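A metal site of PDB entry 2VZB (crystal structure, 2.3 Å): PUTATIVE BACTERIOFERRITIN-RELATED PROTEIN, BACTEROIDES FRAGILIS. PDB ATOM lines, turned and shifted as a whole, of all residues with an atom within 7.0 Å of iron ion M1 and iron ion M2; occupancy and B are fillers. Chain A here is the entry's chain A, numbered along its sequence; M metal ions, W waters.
OE2 of Glu 29 lies close to OH of Tyr 121, 2.5 Å away.
The side-chain carboxylate of Glu 114 sits close to the side-chain hydroxyl of Tyr 36 (2.4 Å).
A ring nitrogen (NE2) of His 149 lies within hydrogen-bond range of the side-chain carboxylate of Glu 61.
The side-chain carboxylate (OE1) of Glu 145 sits at hydrogen-bond distance from a ring nitrogen (NE2) of His 65 (2.7 Å).
O of Glu 61 sits close to NE2 of His 65 (3.4 Å).
Iron ion M1 is bound by the side-chain carboxylate (OE1) of Glu 146 (2.1 Å), the side-chain carboxylate (OE2) of Glu 62 (2.1 Å), the side-chain carboxylate (OE1) of Glu 114 (2.2 Å), a ring nitrogen (ND1) of His 149 (2.3 Å), water W1 (2.3 Å) and the side-chain carboxylate (OE2) of Glu 114 (2.5 Å).
Iron ion M1 has six donor atoms within binding distance.
Iron ion M2 is bound by the side-chain carboxylate (OE1) of Glu 62 (2.0 Å), the side-chain carboxylate (OE2) of Glu 146 (2.1 Å), the side-chain carboxylate (OE1) of Glu 29 (2.2 Å), the side-chain carboxylate (OE2) of Glu 29 (2.2 Å), a ring nitrogen (ND1) of His 65 (2.3 Å) and water W2 (2.5 Å).
Within 4 Å of iron ion M1: Glu 62, Glu 114, Glu 146 and His 149.
The nearest printed residue that does not touch iron ion M1 is Tyr 36 (4.4 Å).
Four residues have an atom within 4 Å of iron ion M2: Glu 29, Glu 62, His 65 and Glu 146.
Along chain A the residues within 4 Å of iron ion M2 span positions 29 to 146.
The nearest printed residue that does not touch iron ion M2 is Ile 142 (4.2 Å).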
ATOM      1  N   ALA A  25     -25.299  27.672  20.219  1.00  0.00           N
ATOM      2  CA  ALA A  25     -24.038  26.886  20.153  1.00  0.00           C
ATOM      3  C   ALA A  25     -24.305  25.369  20.001  1.00  0.00           C
ATOM      4  O   ALA A  25     -23.696  24.696  19.168  1.00  0.00           O
ATOM      5  CB  ALA A  25     -23.213  27.149  21.367  1.00  0.00           C
ATOM      6  N   GLU A  28     -25.491  24.492  16.650  1.00  0.00           N
ATOM      7  CA  GLU A  28     -24.330  24.581  15.745  1.00  0.00           C
ATOM      8  C   GLU A  28     -23.399  23.371  15.826  1.00  0.00           C
ATOM      9  O   GLU A  28     -22.872  22.926  14.813  1.00  0.00           O
ATOM     10  CB  GLU A  28     -23.561  25.881  16.039  1.00  0.00           C
ATOM     11  CG  GLU A  28     -24.313  27.096  15.571  1.00  0.00           C
ATOM     12  CD  GLU A  28     -23.824  28.379  16.165  1.00  0.00           C
ATOM     13  OE1 GLU A  28     -22.916  28.324  17.022  1.00  0.00           O
ATOM     14  OE2 GLU A  28     -24.332  29.444  15.764  1.00  0.00           O
ATOM     15  N   GLU A  29     -23.188  22.867  17.044  1.00  0.00           N
ATOM     16  CA  GLU A  29     -22.331  21.693  17.274  1.00  0.00           C
ATOM     17  C   GLU A  29     -22.898  20.473  16.547  1.00  0.00           C
ATOM     18  O   GLU A  29     -22.181  19.762  15.869  1.00  0.00           O
ATOM     19  CB  GLU A  29     -22.156  21.404  18.775  1.00  0.00           C
ATOM     20  CG  GLU A  29     -21.292  22.445  19.511  1.00  0.00           C
ATOM     21  CD  GLU A  29     -19.846  22.436  19.048  1.00  0.00           C
ATOM     22  OE1 GLU A  29     -19.410  21.437  18.414  1.00  0.00           O
ATOM     23  OE2 GLU A  29     -19.124  23.433  19.318  1.00  0.00           O
ATOM     24  N   ALA A  32     -22.351  20.968  12.810  1.00  0.00           N
ATOM     25  CA  ALA A  32     -20.924  20.774  12.553  1.00  0.00           C
ATOM     26  C   ALA A  32     -20.508  19.303  12.657  1.00  0.00           C
ATOM     27  O   ALA A  32     -19.774  18.787  11.822  1.00  0.00           O
ATOM     28  CB  ALA A  32     -20.100  21.638  13.497  1.00  0.00           C
ATOM     29  N   TYR A  33     -21.043  18.637  13.668  1.00  0.00           N
ATOM     30  CA  TYR A  33     -20.854  17.189  13.883  1.00  0.00           C
ATOM     31  C   TYR A  33     -21.289  16.389  12.663  1.00  0.00           C
ATOM     32  O   TYR A  33     -20.507  15.612  12.102  1.00  0.00           O
ATOM     33  CB  TYR A  33     -21.640  16.788  15.161  1.00  0.00           C
ATOM     34  CG  TYR A  33     -21.758  15.323  15.519  1.00  0.00           C
ATOM     35  CD1 TYR A  33     -20.790  14.392  15.184  1.00  0.00           C
ATOM     36  CD2 TYR A  33     -22.828  14.908  16.302  1.00  0.00           C
ATOM     37  CE1 TYR A  33     -20.934  13.061  15.557  1.00  0.00           C
ATOM     38  CE2 TYR A  33     -22.966  13.599  16.680  1.00  0.00           C
ATOM     39  CZ  TYR A  33     -22.015  12.690  16.302  1.00  0.00           C
ATOM     40  OH  TYR A  33     -22.188  11.396  16.714  1.00  0.00           O
ATOM     41  N   TYR A  36     -19.155  17.151   9.398  1.00  0.00           N
ATOM     42  CA  TYR A  36     -17.889  16.376   9.388  1.00  0.00           C
ATOM     43  C   TYR A  36     -18.120  14.881   9.130  1.00  0.00           C
ATOM     44  O   TYR A  36     -17.377  14.232   8.393  1.00  0.00           O
ATOM     45  CB  TYR A  36     -17.188  16.524  10.720  1.00  0.00           C
ATOM     46  CG  TYR A  36     -16.229  17.672  10.818  1.00  0.00           C
ATOM     47  CD1 TYR A  36     -15.193  17.845   9.899  1.00  0.00           C
ATOM     48  CD2 TYR A  36     -16.318  18.579  11.861  1.00  0.00           C
ATOM     49  CE1 TYR A  36     -14.274  18.894  10.024  1.00  0.00           C
ATOM     50  CE2 TYR A  36     -15.407  19.629  11.991  1.00  0.00           C
ATOM     51  CZ  TYR A  36     -14.404  19.769  11.065  1.00  0.00           C
ATOM     52  OH  TYR A  36     -13.545  20.829  11.207  1.00  0.00           O
ATOM     53  N   HIS A  58     -12.730  15.058  14.121  1.00  0.00           N
ATOM     54  CA  HIS A  58     -13.424  16.315  14.397  1.00  0.00           C
ATOM     55  C   HIS A  58     -14.913  16.113  14.673  1.00  0.00           C
ATOM     56  O   HIS A  58     -15.478  16.740  15.573  1.00  0.00           O
ATOM     57  CB  HIS A  58     -13.180  17.312  13.264  1.00  0.00           C
ATOM     58  CG  HIS A  58     -11.773  17.808  13.212  1.00  0.00           C
ATOM     59  ND1 HIS A  58     -11.400  18.931  12.500  1.00  0.00           N
ATOM     60  CD2 HIS A  58     -10.645  17.369  13.825  1.00  0.00           C
ATOM     61  CE1 HIS A  58     -10.103  19.123  12.646  1.00  0.00           C
ATOM     62  NE2 HIS A  58      -9.622  18.196  13.454  1.00  0.00           N
ATOM     63  N   GLU A  61     -15.041  15.143  18.178  1.00  0.00           N
ATOM     64  CA  GLU A  61     -14.763  16.296  19.046  1.00  0.00           C
ATOM     65  C   GLU A  61     -15.931  17.280  19.164  1.00  0.00           C
ATOM     66  O   GLU A  61     -16.220  17.768  20.244  1.00  0.00           O
ATOM     67  CB  GLU A  61     -13.457  16.982  18.623  1.00  0.00           C
ATOM     68  CG  GLU A  61     -12.253  16.082  18.990  1.00  0.00           C
ATOM     69  CD  GLU A  61     -10.911  16.575  18.506  1.00  0.00           C
ATOM     70  OE1 GLU A  61     -10.824  17.377  17.558  1.00  0.00           O
ATOM     71  OE2 GLU A  61      -9.914  16.116  19.094  1.00  0.00           O
ATOM     72  N   GLU A  62     -16.629  17.531  18.059  1.00  0.00           N
ATOM     73  CA  GLU A  62     -17.843  18.388  18.112  1.00  0.00           C
ATOM     74  C   GLU A  62     -18.932  17.709  18.904  1.00  0.00           C
ATOM     75  O   GLU A  62     -19.652  18.349  19.639  1.00  0.00           O
ATOM     76  CB  GLU A  62     -18.431  18.711  16.720  1.00  0.00           C
ATOM     77  CG  GLU A  62     -17.468  19.138  15.648  1.00  0.00           C
ATOM     78  CD  GLU A  62     -16.669  20.380  16.009  1.00  0.00           C
ATOM     79  OE1 GLU A  62     -16.757  20.903  17.122  1.00  0.00           O
ATOM     80  OE2 GLU A  62     -15.925  20.844  15.128  1.00  0.00           O
ATOM     81  N   ARG A  63     -19.077  16.412  18.703  1.00  0.00           N
ATOM     82  CA  ARG A  63     -20.001  15.599  19.503  1.00  0.00           C
ATOM     83  C   ARG A  63     -19.794  15.800  20.999  1.00  0.00           C
ATOM     84  O   ARG A  63     -20.780  15.948  21.722  1.00  0.00           O
ATOM     85  CB  ARG A  63     -19.831  14.133  19.144  1.00  0.00           C
ATOM     86  CG  ARG A  63     -20.740  13.172  19.914  1.00  0.00           C
ATOM     87  CD  ARG A  63     -22.203  13.572  19.975  1.00  0.00           C
ATOM     88  NE  ARG A  63     -22.929  12.585  20.780  1.00  0.00           N
ATOM     89  CZ  ARG A  63     -23.068  12.648  22.108  1.00  0.00           C
ATOM     90  NH1 ARG A  63     -22.571  13.668  22.817  1.00  0.00           N
ATOM     91  NH2 ARG A  63     -23.728  11.666  22.712  1.00  0.00           N
ATOM     92  N   HIS A  65     -18.243  18.449  22.389  1.00  0.00           N
ATOM     93  CA  HIS A  65     -18.594  19.868  22.641  1.00  0.00           C
ATOM     94  C   HIS A  65     -20.070  20.010  22.957  1.00  0.00           C
ATOM     95  O   HIS A  65     -20.459  20.684  23.907  1.00  0.00           O
ATOM     96  CB  HIS A  65     -18.303  20.761  21.433  1.00  0.00           C
ATOM     97  CG  HIS A  65     -16.858  20.854  21.075  1.00  0.00           C
ATOM     98  ND1 HIS A  65     -16.435  21.367  19.878  1.00  0.00           N
ATOM     99  CD2 HIS A  65     -15.748  20.455  21.743  1.00  0.00           C
ATOM    100  CE1 HIS A  65     -15.110  21.298  19.821  1.00  0.00           C
ATOM    101  NE2 HIS A  65     -14.667  20.754  20.939  1.00  0.00           N
ATOM    102  N   ALA A  66     -20.900  19.365  22.147  1.00  0.00           N
ATOM    103  CA  ALA A  66     -22.360  19.331  22.339  1.00  0.00           C
ATOM    104  C   ALA A  66     -22.750  18.892  23.761  1.00  0.00           C
ATOM    105  O   ALA A  66     -23.638  19.495  24.387  1.00  0.00           O
ATOM    106  CB  ALA A  66     -23.025  18.427  21.312  1.00  0.00           C
ATOM    107  N   ILE A  69     -21.838  21.474  26.436  1.00  0.00           N
ATOM    108  CA  ILE A  69     -22.772  22.594  26.363  1.00  0.00           C
ATOM    109  C   ILE A  69     -24.121  22.201  26.944  1.00  0.00           C
ATOM    110  O   ILE A  69     -24.656  22.873  27.812  1.00  0.00           O
ATOM    111  CB  ILE A  69     -22.946  23.084  24.906  1.00  0.00           C
ATOM    112  CG1 ILE A  69     -21.659  23.748  24.425  1.00  0.00           C
ATOM    113  CG2 ILE A  69     -24.150  24.072  24.784  1.00  0.00           C
ATOM    114  CD1 ILE A  69     -21.570  23.818  22.891  1.00  0.00           C
ATOM    115  N   ASN A 110     -15.636  23.257   5.765  1.00  0.00           N
ATOM    116  CA  ASN A 110     -15.432  23.007   7.198  1.00  0.00           C
ATOM    117  C   ASN A 110     -14.606  24.116   7.871  1.00  0.00           C
ATOM    118  O   ASN A 110     -14.874  24.475   9.014  1.00  0.00           O
ATOM    119  CB  ASN A 110     -14.890  21.607   7.433  1.00  0.00           C
ATOM    120  CG  ASN A 110     -15.939  20.545   7.217  1.00  0.00           C
ATOM    121  OD1 ASN A 110     -16.961  20.547   7.873  1.00  0.00           O
ATOM    122  ND2 ASN A 110     -15.707  19.662   6.266  1.00  0.00           N
ATOM    123  N   SER A 113     -17.128  26.804   8.783  1.00  0.00           N
ATOM    124  CA  SER A 113     -17.881  26.381   9.939  1.00  0.00           C
ATOM    125  C   SER A 113     -17.058  26.591  11.192  1.00  0.00           C
ATOM    126  O   SER A 113     -17.577  27.056  12.194  1.00  0.00           O
ATOM    127  CB  SER A 113     -18.295  24.929   9.781  1.00  0.00           C
ATOM    128  OG  SER A 113     -18.973  24.750   8.554  1.00  0.00           O
ATOM    129  N   GLU A 114     -15.762  26.243  11.116  1.00  0.00           N
ATOM    130  CA  GLU A 114     -14.824  26.459  12.219  1.00  0.00           C
ATOM    131  C   GLU A 114     -14.693  27.909  12.637  1.00  0.00           C
ATOM    132  O   GLU A 114     -14.732  28.222  13.811  1.00  0.00           O
ATOM    133  CB  GLU A 114     -13.417  25.941  11.872  1.00  0.00           C
ATOM    134  CG  GLU A 114     -13.305  24.448  11.763  1.00  0.00           C
ATOM    135  CD  GLU A 114     -13.806  23.679  12.973  1.00  0.00           C
ATOM    136  OE1 GLU A 114     -13.725  24.195  14.115  1.00  0.00           O
ATOM    137  OE2 GLU A 114     -14.262  22.532  12.767  1.00  0.00           O
ATOM    138  N   ALA A 117     -17.565  28.940  14.501  1.00  0.00           N
ATOM    139  CA  ALA A 117     -17.490  28.353  15.851  1.00  0.00           C
ATOM    140  C   ALA A 117     -16.549  29.145  16.762  1.00  0.00           C
ATOM    141  O   ALA A 117     -16.869  29.411  17.913  1.00  0.00           O
ATOM    142  CB  ALA A 117     -17.069  26.879  15.774  1.00  0.00           C
ATOM    143  N   TYR A 121     -17.621  31.009  20.483  1.00  0.00           N
ATOM    144  CA  TYR A 121     -17.046  30.712  21.803  1.00  0.00           C
ATOM    145  C   TYR A 121     -16.289  31.900  22.371  1.00  0.00           C
ATOM    146  O   TYR A 121     -16.270  32.101  23.589  1.00  0.00           O
ATOM    147  CB  TYR A 121     -16.277  29.373  21.831  1.00  0.00           C
ATOM    148  CG  TYR A 121     -17.246  28.271  21.489  1.00  0.00           C
ATOM    149  CD1 TYR A 121     -18.326  27.979  22.328  1.00  0.00           C
ATOM    150  CD2 TYR A 121     -17.171  27.609  20.290  1.00  0.00           C
ATOM    151  CE1 TYR A 121     -19.244  27.034  22.003  1.00  0.00           C
ATOM    152  CE2 TYR A 121     -18.101  26.651  19.951  1.00  0.00           C
ATOM    153  CZ  TYR A 121     -19.142  26.374  20.808  1.00  0.00           C
ATOM    154  OH  TYR A 121     -20.073  25.409  20.484  1.00  0.00           O
ATOM    155  N   ILE A 142     -13.623  24.636  24.482  1.00  0.00           N
ATOM    156  CA  ILE A 142     -14.165  24.391  23.143  1.00  0.00           C
ATOM    157  C   ILE A 142     -13.451  25.277  22.129  1.00  0.00           C
ATOM    158  O   ILE A 142     -12.966  24.809  21.114  1.00  0.00           O
ATOM    159  CB  ILE A 142     -15.700  24.615  23.093  1.00  0.00           C
ATOM    160  CG1 ILE A 142     -16.391  23.663  24.080  1.00  0.00           C
ATOM    161  CG2 ILE A 142     -16.247  24.415  21.673  1.00  0.00           C
ATOM    162  CD1 ILE A 142     -17.889  23.755  24.133  1.00  0.00           C
ATOM    163  N   GLU A 145     -10.083  24.062  21.012  1.00  0.00           N
ATOM    164  CA  GLU A 145     -10.258  22.966  20.056  1.00  0.00           C
ATOM    165  C   GLU A 145     -10.663  23.459  18.655  1.00  0.00           C
ATOM    166  O   GLU A 145     -10.176  22.932  17.652  1.00  0.00           O
ATOM    167  CB  GLU A 145     -11.245  21.905  20.578  1.00  0.00           C
ATOM    168  CG  GLU A 145     -10.725  21.214  21.873  1.00  0.00           C
ATOM    169  CD  GLU A 145     -11.346  19.856  22.152  1.00  0.00           C
ATOM    170  OE1 GLU A 145     -12.398  19.531  21.575  1.00  0.00           O
ATOM    171  OE2 GLU A 145     -10.746  19.131  22.979  1.00  0.00           O
ATOM    172  N   GLU A 146     -11.540  24.450  18.594  1.00  0.00           N
ATOM    173  CA  GLU A 146     -11.997  24.978  17.287  1.00  0.00           C
ATOM    174  C   GLU A 146     -10.842  25.647  16.537  1.00  0.00           C
ATOM    175  O   GLU A 146     -10.729  25.503  15.322  1.00  0.00           O
ATOM    176  CB  GLU A 146     -13.159  25.964  17.413  1.00  0.00           C
ATOM    177  CG  GLU A 146     -14.331  25.563  18.345  1.00  0.00           C
ATOM    178  CD  GLU A 146     -15.101  24.370  17.863  1.00  0.00           C
ATOM    179  OE1 GLU A 146     -14.623  23.678  16.954  1.00  0.00           O
ATOM    180  OE2 GLU A 146     -16.203  24.130  18.391  1.00  0.00           O
ATOM    181  N   GLU A 147      -9.989  26.360  17.266  1.00  0.00           N
ATOM    182  CA  GLU A 147      -8.782  26.951  16.684  1.00  0.00           C
ATOM    183  C   GLU A 147      -7.839  25.878  16.145  1.00  0.00           C
ATOM    184  O   GLU A 147      -7.196  26.075  15.107  1.00  0.00           O
ATOM    185  CB  GLU A 147      -8.035  27.807  17.711  1.00  0.00           C
ATOM    186  CG  GLU A 147      -8.799  29.028  18.186  1.00  0.00           C
ATOM    187  CD  GLU A 147      -7.938  29.987  18.980  1.00  0.00           C
ATOM    188  OE1 GLU A 147      -6.919  30.460  18.462  1.00  0.00           O
ATOM    189  OE2 GLU A 147      -8.275  30.295  20.136  1.00  0.00           O
ATOM    190  N   HIS A 149      -8.820  22.819  15.155  1.00  0.00           N
ATOM    191  CA  HIS A 149      -9.540  22.303  13.983  1.00  0.00           C
ATOM    192  C   HIS A 149      -9.274  23.162  12.762  1.00  0.00           C
ATOM    193  O   HIS A 149      -9.017  22.631  11.678  1.00  0.00           O
ATOM    194  CB  HIS A 149     -11.062  22.310  14.186  1.00  0.00           C
ATOM    195  CG  HIS A 149     -11.563  21.268  15.139  1.00  0.00           C
ATOM    196  ND1 HIS A 149     -12.873  21.246  15.572  1.00  0.00           N
ATOM    197  CD2 HIS A 149     -10.932  20.240  15.758  1.00  0.00           C
ATOM    198  CE1 HIS A 149     -13.027  20.236  16.401  1.00  0.00           C
ATOM    199  NE2 HIS A 149     -11.877  19.612  16.520  1.00  0.00           N
ATOM    200  N   GLU A 150      -9.389  24.472  12.926  1.00  0.00           N
ATOM    201  CA  GLU A 150      -9.102  25.406  11.826  1.00  0.00           C
ATOM    202  C   GLU A 150      -7.700  25.176  11.280  1.00  0.00           C
ATOM    203  O   GLU A 150      -7.523  25.015  10.072  1.00  0.00           O
ATOM    204  CB  GLU A 150      -9.243  26.901  12.221  1.00  0.00           C
ATOM    205  CG  GLU A 150      -9.359  27.759  10.968  1.00  0.00           C
ATOM    206  CD  GLU A 150      -8.871  29.201  11.111  1.00  0.00           C
ATOM    207  OE1 GLU A 150      -8.741  29.738  12.249  1.00  0.00           O
ATOM    208  OE2 GLU A 150      -8.642  29.799  10.027  1.00  0.00           O
HETATM  209 FE    FE M   1     -14.682  22.545  15.237  1.00  0.00          FE
HETATM  210 FE    FE M   2     -17.488  22.440  18.186  1.00  0.00          FE
HETATM  211  O   HOH W   1     -16.494  23.791  14.460  1.00  0.00           O
HETATM  212  O   HOH W   2     -18.572  23.097  16.026  1.00  0.00           O
